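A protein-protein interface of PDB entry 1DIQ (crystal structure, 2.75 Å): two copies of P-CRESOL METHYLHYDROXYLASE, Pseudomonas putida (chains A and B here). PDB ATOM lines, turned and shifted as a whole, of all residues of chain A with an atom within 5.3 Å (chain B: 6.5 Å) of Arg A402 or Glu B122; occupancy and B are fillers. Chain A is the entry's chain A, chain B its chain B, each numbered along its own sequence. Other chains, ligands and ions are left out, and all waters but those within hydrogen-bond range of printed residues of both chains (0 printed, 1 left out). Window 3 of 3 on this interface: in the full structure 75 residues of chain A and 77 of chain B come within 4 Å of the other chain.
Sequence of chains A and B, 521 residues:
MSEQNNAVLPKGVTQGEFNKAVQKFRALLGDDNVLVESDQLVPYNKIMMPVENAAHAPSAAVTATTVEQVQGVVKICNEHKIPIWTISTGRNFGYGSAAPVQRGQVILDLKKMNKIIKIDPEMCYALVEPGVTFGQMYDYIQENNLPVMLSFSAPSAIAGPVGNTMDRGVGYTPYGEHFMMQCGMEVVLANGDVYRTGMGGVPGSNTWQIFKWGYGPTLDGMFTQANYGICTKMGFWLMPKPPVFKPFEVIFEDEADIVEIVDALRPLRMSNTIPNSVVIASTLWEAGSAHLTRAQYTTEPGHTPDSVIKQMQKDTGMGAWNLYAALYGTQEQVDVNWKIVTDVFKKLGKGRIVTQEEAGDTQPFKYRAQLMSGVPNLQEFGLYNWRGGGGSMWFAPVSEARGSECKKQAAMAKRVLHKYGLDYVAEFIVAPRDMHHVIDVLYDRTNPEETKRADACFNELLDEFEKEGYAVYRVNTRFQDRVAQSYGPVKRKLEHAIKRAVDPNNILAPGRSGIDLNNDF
SD of Met A270 lies within hydrogen-bond range of SG of Cys B124, at 3.7 Å. The guanidinium group of Arg A402 lies within salt-bridge range of the side-chain carboxylate of Asp B120 (3.5 Å). NH1 of Arg A402 is in salt-bridge range of OE1 of Glu B122 (3.0 Å). The side-chain amide nitrogen (ND2) of Asn B206 is in hydrogen-bond range of the side-chain carboxylate (OE2) of Glu A405 (3.5 Å).
OD1 of Asp A263 lies within salt-bridge range of NH1 of Arg A266. NH1 of Arg A266 lies within hydrogen-bond range of O of Ala A401 (2.8 Å). NE of Arg A402 lies within salt-bridge range of OE2 of Glu A400 (3.0 Å). The side-chain carboxylate (OD1) of Asp B120 sits at hydrogen-bond distance from the backbone NH (N) of Glu B122, at 3.2 Å. OD1 of Asp B120 sits at hydrogen-bond distance from N of Met B123 (3.0 Å). O of Tyr B125 is in hydrogen-bond range of N of Asp B120, 3.0 Å away.
Glu B122 touches Arg A266 (O to NE, 3.7 Å). Arg A266 touches Met B123. Met B123 touches Met A270. Glu A400 touches Met B123. OE2 of Glu A400 touches ND2 of Asn B206, 3.7 Å away. Met B123 touches Ala A401. NH2 of Arg A402 touches CG of Met B123, at 3.4 Å.
Of the printed residues of chain B, Met A270 touches Met B123 (3.8 Å) and Cys B124 (3.7 Å). Printed residues of chain B within 4 Å of Glu A400: Met B123 (3.7 Å) and Asn B206 (3.7 Å). Of the printed residues of chain B, Ala A401 touches Met B123. Of chain B, only Asp B120, Glu B122 and Met B123 come within 4 Å of Arg A402. Glu B122 touches just these residues of chain A: Arg A266 and Arg A402. Printed residues of chain A within 4 Å of Cys B124: Met A270 (3.7 Å). The nearest printed residue of chain A that does not touch Met B123 is Asp A263 (7.0 Å).
Hydrophobic or aromatic side chains of chain B within 4 Å of the printed part of chain A: Met B123. Of the 11 printed residues of chain A, 6 touch a printed residue of chain B. Printed residues of chain A that touch a printed residue of chain B: Arg A266, Met A270, Glu A400, Ala A401, Arg A402 and Glu A405. Among the printed residues, 11 pairs touch across the chains. Among the printed residues, Asp or Glu carboxylates within 4 Å of a Lys or Arg side-chain nitrogen of the other chain: Arg A402 with Asp B120 and Arg A402 with Glu B122.
No position is printed for both chains. Of the 11 pairs that touch across the chains among the printed residues, none has its exchanged pair printed and touching as well.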
ATOM      1  N   VAL A 262      10.014  -9.533  -4.727  1.00  0.00           N
ATOM      2  CA  VAL A 262       9.174  -8.569  -5.411  1.00  0.00           C
ATOM      3  C   VAL A 262       8.194  -9.238  -6.369  1.00  0.00           C
ATOM      4  O   VAL A 262       6.992  -8.985  -6.283  1.00  0.00           O
ATOM      5  CB  VAL A 262      10.036  -7.519  -6.135  1.00  0.00           C
ATOM      6  CG1 VAL A 262       9.194  -6.538  -6.889  1.00  0.00           C
ATOM      7  CG2 VAL A 262      10.895  -6.785  -5.149  1.00  0.00           C
ATOM      8  N   ASP A 263       8.704 -10.150  -7.205  1.00  0.00           N
ATOM      9  CA  ASP A 263       7.897 -10.877  -8.192  1.00  0.00           C
ATOM     10  C   ASP A 263       6.851 -11.811  -7.591  1.00  0.00           C
ATOM     11  O   ASP A 263       5.807 -12.033  -8.184  1.00  0.00           O
ATOM     12  CB  ASP A 263       8.797 -11.623  -9.178  1.00  0.00           C
ATOM     13  CG  ASP A 263       9.521 -10.683 -10.160  1.00  0.00           C
ATOM     14  OD1 ASP A 263       9.294  -9.454 -10.142  1.00  0.00           O
ATOM     15  OD2 ASP A 263      10.333 -11.179 -10.970  1.00  0.00           O
ATOM     16  N   ARG A 266       4.033  -9.222  -5.745  1.00  0.00           N
ATOM     17  CA  ARG A 266       3.192  -8.487  -6.683  1.00  0.00           C
ATOM     18  C   ARG A 266       1.760  -9.006  -6.872  1.00  0.00           C
ATOM     19  O   ARG A 266       0.825  -8.217  -6.696  1.00  0.00           O
ATOM     20  CB  ARG A 266       3.931  -8.234  -8.014  1.00  0.00           C
ATOM     21  CG  ARG A 266       3.183  -7.358  -8.996  1.00  0.00           C
ATOM     22  CD  ARG A 266       3.959  -7.122 -10.271  1.00  0.00           C
ATOM     23  NE  ARG A 266       4.260  -8.355 -10.993  1.00  0.00           N
ATOM     24  CZ  ARG A 266       5.482  -8.853 -11.150  1.00  0.00           C
ATOM     25  NH1 ARG A 266       6.531  -8.234 -10.630  1.00  0.00           N
ATOM     26  NH2 ARG A 266       5.654  -9.967 -11.837  1.00  0.00           N
ATOM     27  N   MET A 270      -1.590  -6.784  -5.829  1.00  0.00           N
ATOM     28  CA  MET A 270      -2.534  -6.473  -6.897  1.00  0.00           C
ATOM     29  C   MET A 270      -3.937  -7.012  -6.675  1.00  0.00           C
ATOM     30  O   MET A 270      -4.916  -6.341  -7.006  1.00  0.00           O
ATOM     31  CB  MET A 270      -1.983  -6.948  -8.234  1.00  0.00           C
ATOM     32  CG  MET A 270      -2.238  -5.948  -9.308  1.00  0.00           C
ATOM     33  SD  MET A 270      -1.220  -6.181 -10.704  1.00  0.00           S
ATOM     34  CE  MET A 270       0.111  -5.281 -10.274  1.00  0.00           C
ATOM     35  N   GLU A 400       9.180   0.293 -11.056  1.00  0.00           N
ATOM     36  CA  GLU A 400       8.148  -0.679 -11.385  1.00  0.00           C
ATOM     37  C   GLU A 400       8.262  -1.761 -10.289  1.00  0.00           C
ATOM     38  O   GLU A 400       9.373  -2.057  -9.826  1.00  0.00           O
ATOM     39  CB  GLU A 400       8.559  -1.268 -12.732  1.00  0.00           C
ATOM     40  CG  GLU A 400       7.474  -1.766 -13.646  1.00  0.00           C
ATOM     41  CD  GLU A 400       7.990  -2.082 -15.056  1.00  0.00           C
ATOM     42  OE1 GLU A 400       7.189  -1.976 -16.002  1.00  0.00           O
ATOM     43  OE2 GLU A 400       9.182  -2.443 -15.231  1.00  0.00           O
ATOM     44  N   ALA A 401       7.137  -2.304  -9.825  1.00  0.00           N
ATOM     45  CA  ALA A 401       7.165  -3.378  -8.813  1.00  0.00           C
ATOM     46  C   ALA A 401       7.486  -4.695  -9.523  1.00  0.00           C
ATOM     47  O   ALA A 401       6.708  -5.646  -9.520  1.00  0.00           O
ATOM     48  CB  ALA A 401       5.843  -3.477  -8.069  1.00  0.00           C
ATOM     49  N   ARG A 402       8.645  -4.687 -10.174  1.00  0.00           N
ATOM     50  CA  ARG A 402       9.179  -5.803 -10.926  1.00  0.00           C
ATOM     51  C   ARG A 402      10.577  -6.007 -10.350  1.00  0.00           C
ATOM     52  O   ARG A 402      11.368  -5.061 -10.278  1.00  0.00           O
ATOM     53  CB  ARG A 402       9.252  -5.434 -12.408  1.00  0.00           C
ATOM     54  CG  ARG A 402       9.478  -6.609 -13.335  1.00  0.00           C
ATOM     55  CD  ARG A 402       9.891  -6.143 -14.724  1.00  0.00           C
ATOM     56  NE  ARG A 402       8.852  -5.396 -15.437  1.00  0.00           N
ATOM     57  CZ  ARG A 402       7.810  -5.939 -16.076  1.00  0.00           C
ATOM     58  NH1 ARG A 402       7.620  -7.261 -16.096  1.00  0.00           N
ATOM     59  NH2 ARG A 402       6.986  -5.153 -16.762  1.00  0.00           N
ATOM     60  N   GLY A 403      10.846  -7.242  -9.921  1.00  0.00           N
ATOM     61  CA  GLY A 403      12.117  -7.627  -9.315  1.00  0.00           C
ATOM     62  C   GLY A 403      13.458  -7.283  -9.942  1.00  0.00           C
ATOM     63  O   GLY A 403      14.395  -6.940  -9.227  1.00  0.00           O
ATOM     64  N   SER A 404      13.559  -7.400 -11.265  1.00  0.00           N
ATOM     65  CA  SER A 404      14.789  -7.095 -11.973  1.00  0.00           C
ATOM     66  C   SER A 404      15.131  -5.603 -11.878  1.00  0.00           C
ATOM     67  O   SER A 404      16.305  -5.232 -11.800  1.00  0.00           O
ATOM     68  CB  SER A 404      14.667  -7.528 -13.438  1.00  0.00           C
ATOM     69  OG  SER A 404      13.730  -6.724 -14.137  1.00  0.00           O
ATOM     70  N   GLU A 405      14.083  -4.772 -11.829  1.00  0.00           N
ATOM     71  CA  GLU A 405      14.194  -3.310 -11.751  1.00  0.00           C
ATOM     72  C   GLU A 405      14.666  -2.853 -10.390  1.00  0.00           C
ATOM     73  O   GLU A 405      15.482  -1.927 -10.284  1.00  0.00           O
ATOM     74  CB  GLU A 405      12.852  -2.646 -12.074  1.00  0.00           C
ATOM     75  CG  GLU A 405      12.480  -2.649 -13.549  1.00  0.00           C
ATOM     76  CD  GLU A 405      13.443  -1.825 -14.403  1.00  0.00           C
ATOM     77  OE1 GLU A 405      14.102  -2.424 -15.292  1.00  0.00           O
ATOM     78  OE2 GLU A 405      13.542  -0.592 -14.176  1.00  0.00           O
ATOM     79  N   CYS A 406      14.190  -3.554  -9.361  1.00  0.00           N
ATOM     80  CA  CYS A 406      14.536  -3.258  -7.979  1.00  0.00           C
ATOM     81  C   CYS A 406      16.014  -3.580  -7.734  1.00  0.00           C
ATOM     82  O   CYS A 406      16.745  -2.768  -7.156  1.00  0.00           O
ATOM     83  CB  CYS A 406      13.611  -4.039  -7.038  1.00  0.00           C
ATOM     84  SG  CYS A 406      11.891  -3.394  -6.979  1.00  0.00           S
ATOM     85  N   LYS B 118      -0.036  -0.601 -25.925  1.00  0.00           N
ATOM     86  CA  LYS B 118       0.561  -1.592 -25.027  1.00  0.00           C
ATOM     87  C   LYS B 118      -0.452  -2.073 -23.995  1.00  0.00           C
ATOM     88  O   LYS B 118      -1.304  -1.303 -23.549  1.00  0.00           O
ATOM     89  CB  LYS B 118       1.756  -0.946 -24.274  1.00  0.00           C
ATOM     90  CG  LYS B 118       2.730  -1.887 -23.551  1.00  0.00           C
ATOM     91  CD  LYS B 118       3.930  -1.075 -23.019  1.00  0.00           C
ATOM     92  CE  LYS B 118       5.124  -1.945 -22.560  1.00  0.00           C
ATOM     93  NZ  LYS B 118       4.915  -2.729 -21.298  1.00  0.00           N
ATOM     94  N   ILE B 119      -0.431  -3.374 -23.722  1.00  0.00           N
ATOM     95  CA  ILE B 119      -1.250  -3.966 -22.668  1.00  0.00           C
ATOM     96  C   ILE B 119      -0.233  -4.883 -22.016  1.00  0.00           C
ATOM     97  O   ILE B 119       0.230  -5.849 -22.630  1.00  0.00           O
ATOM     98  CB  ILE B 119      -2.510  -4.762 -23.144  1.00  0.00           C
ATOM     99  CG1 ILE B 119      -3.562  -3.811 -23.729  1.00  0.00           C
ATOM    100  CG2 ILE B 119      -3.164  -5.477 -21.940  1.00  0.00           C
ATOM    101  CD1 ILE B 119      -4.846  -4.473 -24.225  1.00  0.00           C
ATOM    102  N   ASP B 120       0.200  -4.505 -20.818  1.00  0.00           N
ATOM    103  CA  ASP B 120       1.187  -5.272 -20.060  1.00  0.00           C
ATOM    104  C   ASP B 120       0.436  -6.260 -19.149  1.00  0.00           C
ATOM    105  O   ASP B 120      -0.238  -5.843 -18.214  1.00  0.00           O
ATOM    106  CB  ASP B 120       2.026  -4.293 -19.250  1.00  0.00           C
ATOM    107  CG  ASP B 120       3.292  -4.903 -18.701  1.00  0.00           C
ATOM    108  OD1 ASP B 120       3.194  -5.959 -18.020  1.00  0.00           O
ATOM    109  OD2 ASP B 120       4.372  -4.293 -18.931  1.00  0.00           O
ATOM    110  N   PRO B 121       0.532  -7.578 -19.426  1.00  0.00           N
ATOM    111  CA  PRO B 121      -0.179  -8.560 -18.586  1.00  0.00           C
ATOM    112  C   PRO B 121       0.364  -8.823 -17.174  1.00  0.00           C
ATOM    113  O   PRO B 121      -0.385  -9.269 -16.302  1.00  0.00           O
ATOM    114  CB  PRO B 121      -0.193  -9.810 -19.463  1.00  0.00           C
ATOM    115  CG  PRO B 121       1.107  -9.680 -20.252  1.00  0.00           C
ATOM    116  CD  PRO B 121       1.139  -8.227 -20.611  1.00  0.00           C
ATOM    117  N   GLU B 122       1.643  -8.511 -16.947  1.00  0.00           N
ATOM    118  CA  GLU B 122       2.284  -8.702 -15.631  1.00  0.00           C
ATOM    119  C   GLU B 122       2.041  -7.518 -14.689  1.00  0.00           C
ATOM    120  O   GLU B 122       1.646  -7.699 -13.527  1.00  0.00           O
ATOM    121  CB  GLU B 122       3.792  -8.919 -15.794  1.00  0.00           C
ATOM    122  CG  GLU B 122       4.214 -10.327 -16.201  1.00  0.00           C
ATOM    123  CD  GLU B 122       5.565 -10.332 -16.903  1.00  0.00           C
ATOM    124  OE1 GLU B 122       6.596 -10.103 -16.225  1.00  0.00           O
ATOM    125  OE2 GLU B 122       5.591 -10.544 -18.140  1.00  0.00           O
ATOM    126  N   MET B 123       2.289  -6.311 -15.203  1.00  0.00           N
ATOM    127  CA  MET B 123       2.083  -5.081 -14.447  1.00  0.00           C
ATOM    128  C   MET B 123       0.640  -4.606 -14.455  1.00  0.00           C
ATOM    129  O   MET B 123       0.303  -3.672 -13.742  1.00  0.00           O
ATOM    130  CB  MET B 123       2.990  -3.953 -14.947  1.00  0.00           C
ATOM    131  CG  MET B 123       4.485  -4.153 -14.743  1.00  0.00           C
ATOM    132  SD  MET B 123       5.034  -4.813 -13.127  1.00  0.00           S
ATOM    133  CE  MET B 123       4.520  -3.598 -12.001  1.00  0.00           C
ATOM    134  N   CYS B 124      -0.189  -5.247 -15.287  1.00  0.00           N
ATOM    135  CA  CYS B 124      -1.618  -4.962 -15.434  1.00  0.00           C
ATOM    136  C   CYS B 124      -2.017  -3.514 -15.707  1.00  0.00           C
ATOM    137  O   CYS B 124      -2.588  -2.834 -14.848  1.00  0.00           O
ATOM    138  CB  CYS B 124      -2.399  -5.532 -14.252  1.00  0.00           C
ATOM    139  SG  CYS B 124      -2.165  -7.273 -14.096  1.00  0.00           S
ATOM    140  N   TYR B 125      -1.639  -3.047 -16.895  1.00  0.00           N
ATOM    141  CA  TYR B 125      -1.958  -1.709 -17.359  1.00  0.00           C
ATOM    142  C   TYR B 125      -2.201  -1.684 -18.868  1.00  0.00           C
ATOM    143  O   TYR B 125      -1.824  -2.615 -19.576  1.00  0.00           O
ATOM    144  CB  TYR B 125      -0.882  -0.689 -16.931  1.00  0.00           C
ATOM    145  CG  TYR B 125       0.482  -0.748 -17.602  1.00  0.00           C
ATOM    146  CD1 TYR B 125       0.659  -0.339 -18.950  1.00  0.00           C
ATOM    147  CD2 TYR B 125       1.628  -1.098 -16.869  1.00  0.00           C
ATOM    148  CE1 TYR B 125       1.934  -0.271 -19.550  1.00  0.00           C
ATOM    149  CE2 TYR B 125       2.932  -1.030 -17.461  1.00  0.00           C
ATOM    150  CZ  TYR B 125       3.059  -0.613 -18.803  1.00  0.00           C
ATOM    151  OH  TYR B 125       4.288  -0.516 -19.401  1.00  0.00           O
ATOM    152  N   PRO B 147      -4.531 -12.411 -18.994  1.00  0.00           N
ATOM    153  CA  PRO B 147      -5.286 -12.553 -17.734  1.00  0.00           C
ATOM    154  C   PRO B 147      -5.777 -11.240 -17.075  1.00  0.00           C
ATOM    155  O   PRO B 147      -5.775 -11.099 -15.846  1.00  0.00           O
ATOM    156  CB  PRO B 147      -4.315 -13.355 -16.849  1.00  0.00           C
ATOM    157  CG  PRO B 147      -2.972 -12.807 -17.264  1.00  0.00           C
ATOM    158  CD  PRO B 147      -3.085 -12.646 -18.776  1.00  0.00           C
ATOM    159  N   VAL B 148      -6.202 -10.290 -17.904  1.00  0.00           N
ATOM    160  CA  VAL B 148      -6.710  -9.006 -17.421  1.00  0.00           C
ATOM    161  C   VAL B 148      -8.215  -8.877 -17.643  1.00  0.00           C
ATOM    162  O   VAL B 148      -8.791  -9.539 -18.505  1.00  0.00           O
ATOM    163  CB  VAL B 148      -5.952  -7.781 -18.034  1.00  0.00           C
ATOM    164  CG1 VAL B 148      -4.531  -7.735 -17.537  1.00  0.00           C
ATOM    165  CG2 VAL B 148      -5.940  -7.824 -19.526  1.00  0.00           C
ATOM    166  N   ASN B 206       9.952   4.073 -18.035  1.00  0.00           N
ATOM    167  CA  ASN B 206       9.131   2.871 -18.174  1.00  0.00           C
ATOM    168  C   ASN B 206       8.092   2.857 -17.053  1.00  0.00           C
ATOM    169  O   ASN B 206       7.481   1.827 -16.767  1.00  0.00           O
ATOM    170  CB  ASN B 206       9.999   1.594 -18.160  1.00  0.00           C
ATOM    171  CG  ASN B 206      10.763   1.368 -16.837  1.00  0.00           C
ATOM    172  OD1 ASN B 206      10.864   2.244 -15.963  1.00  0.00           O
ATOM    173  ND2 ASN B 206      11.303   0.166 -16.701  1.00  0.00           N
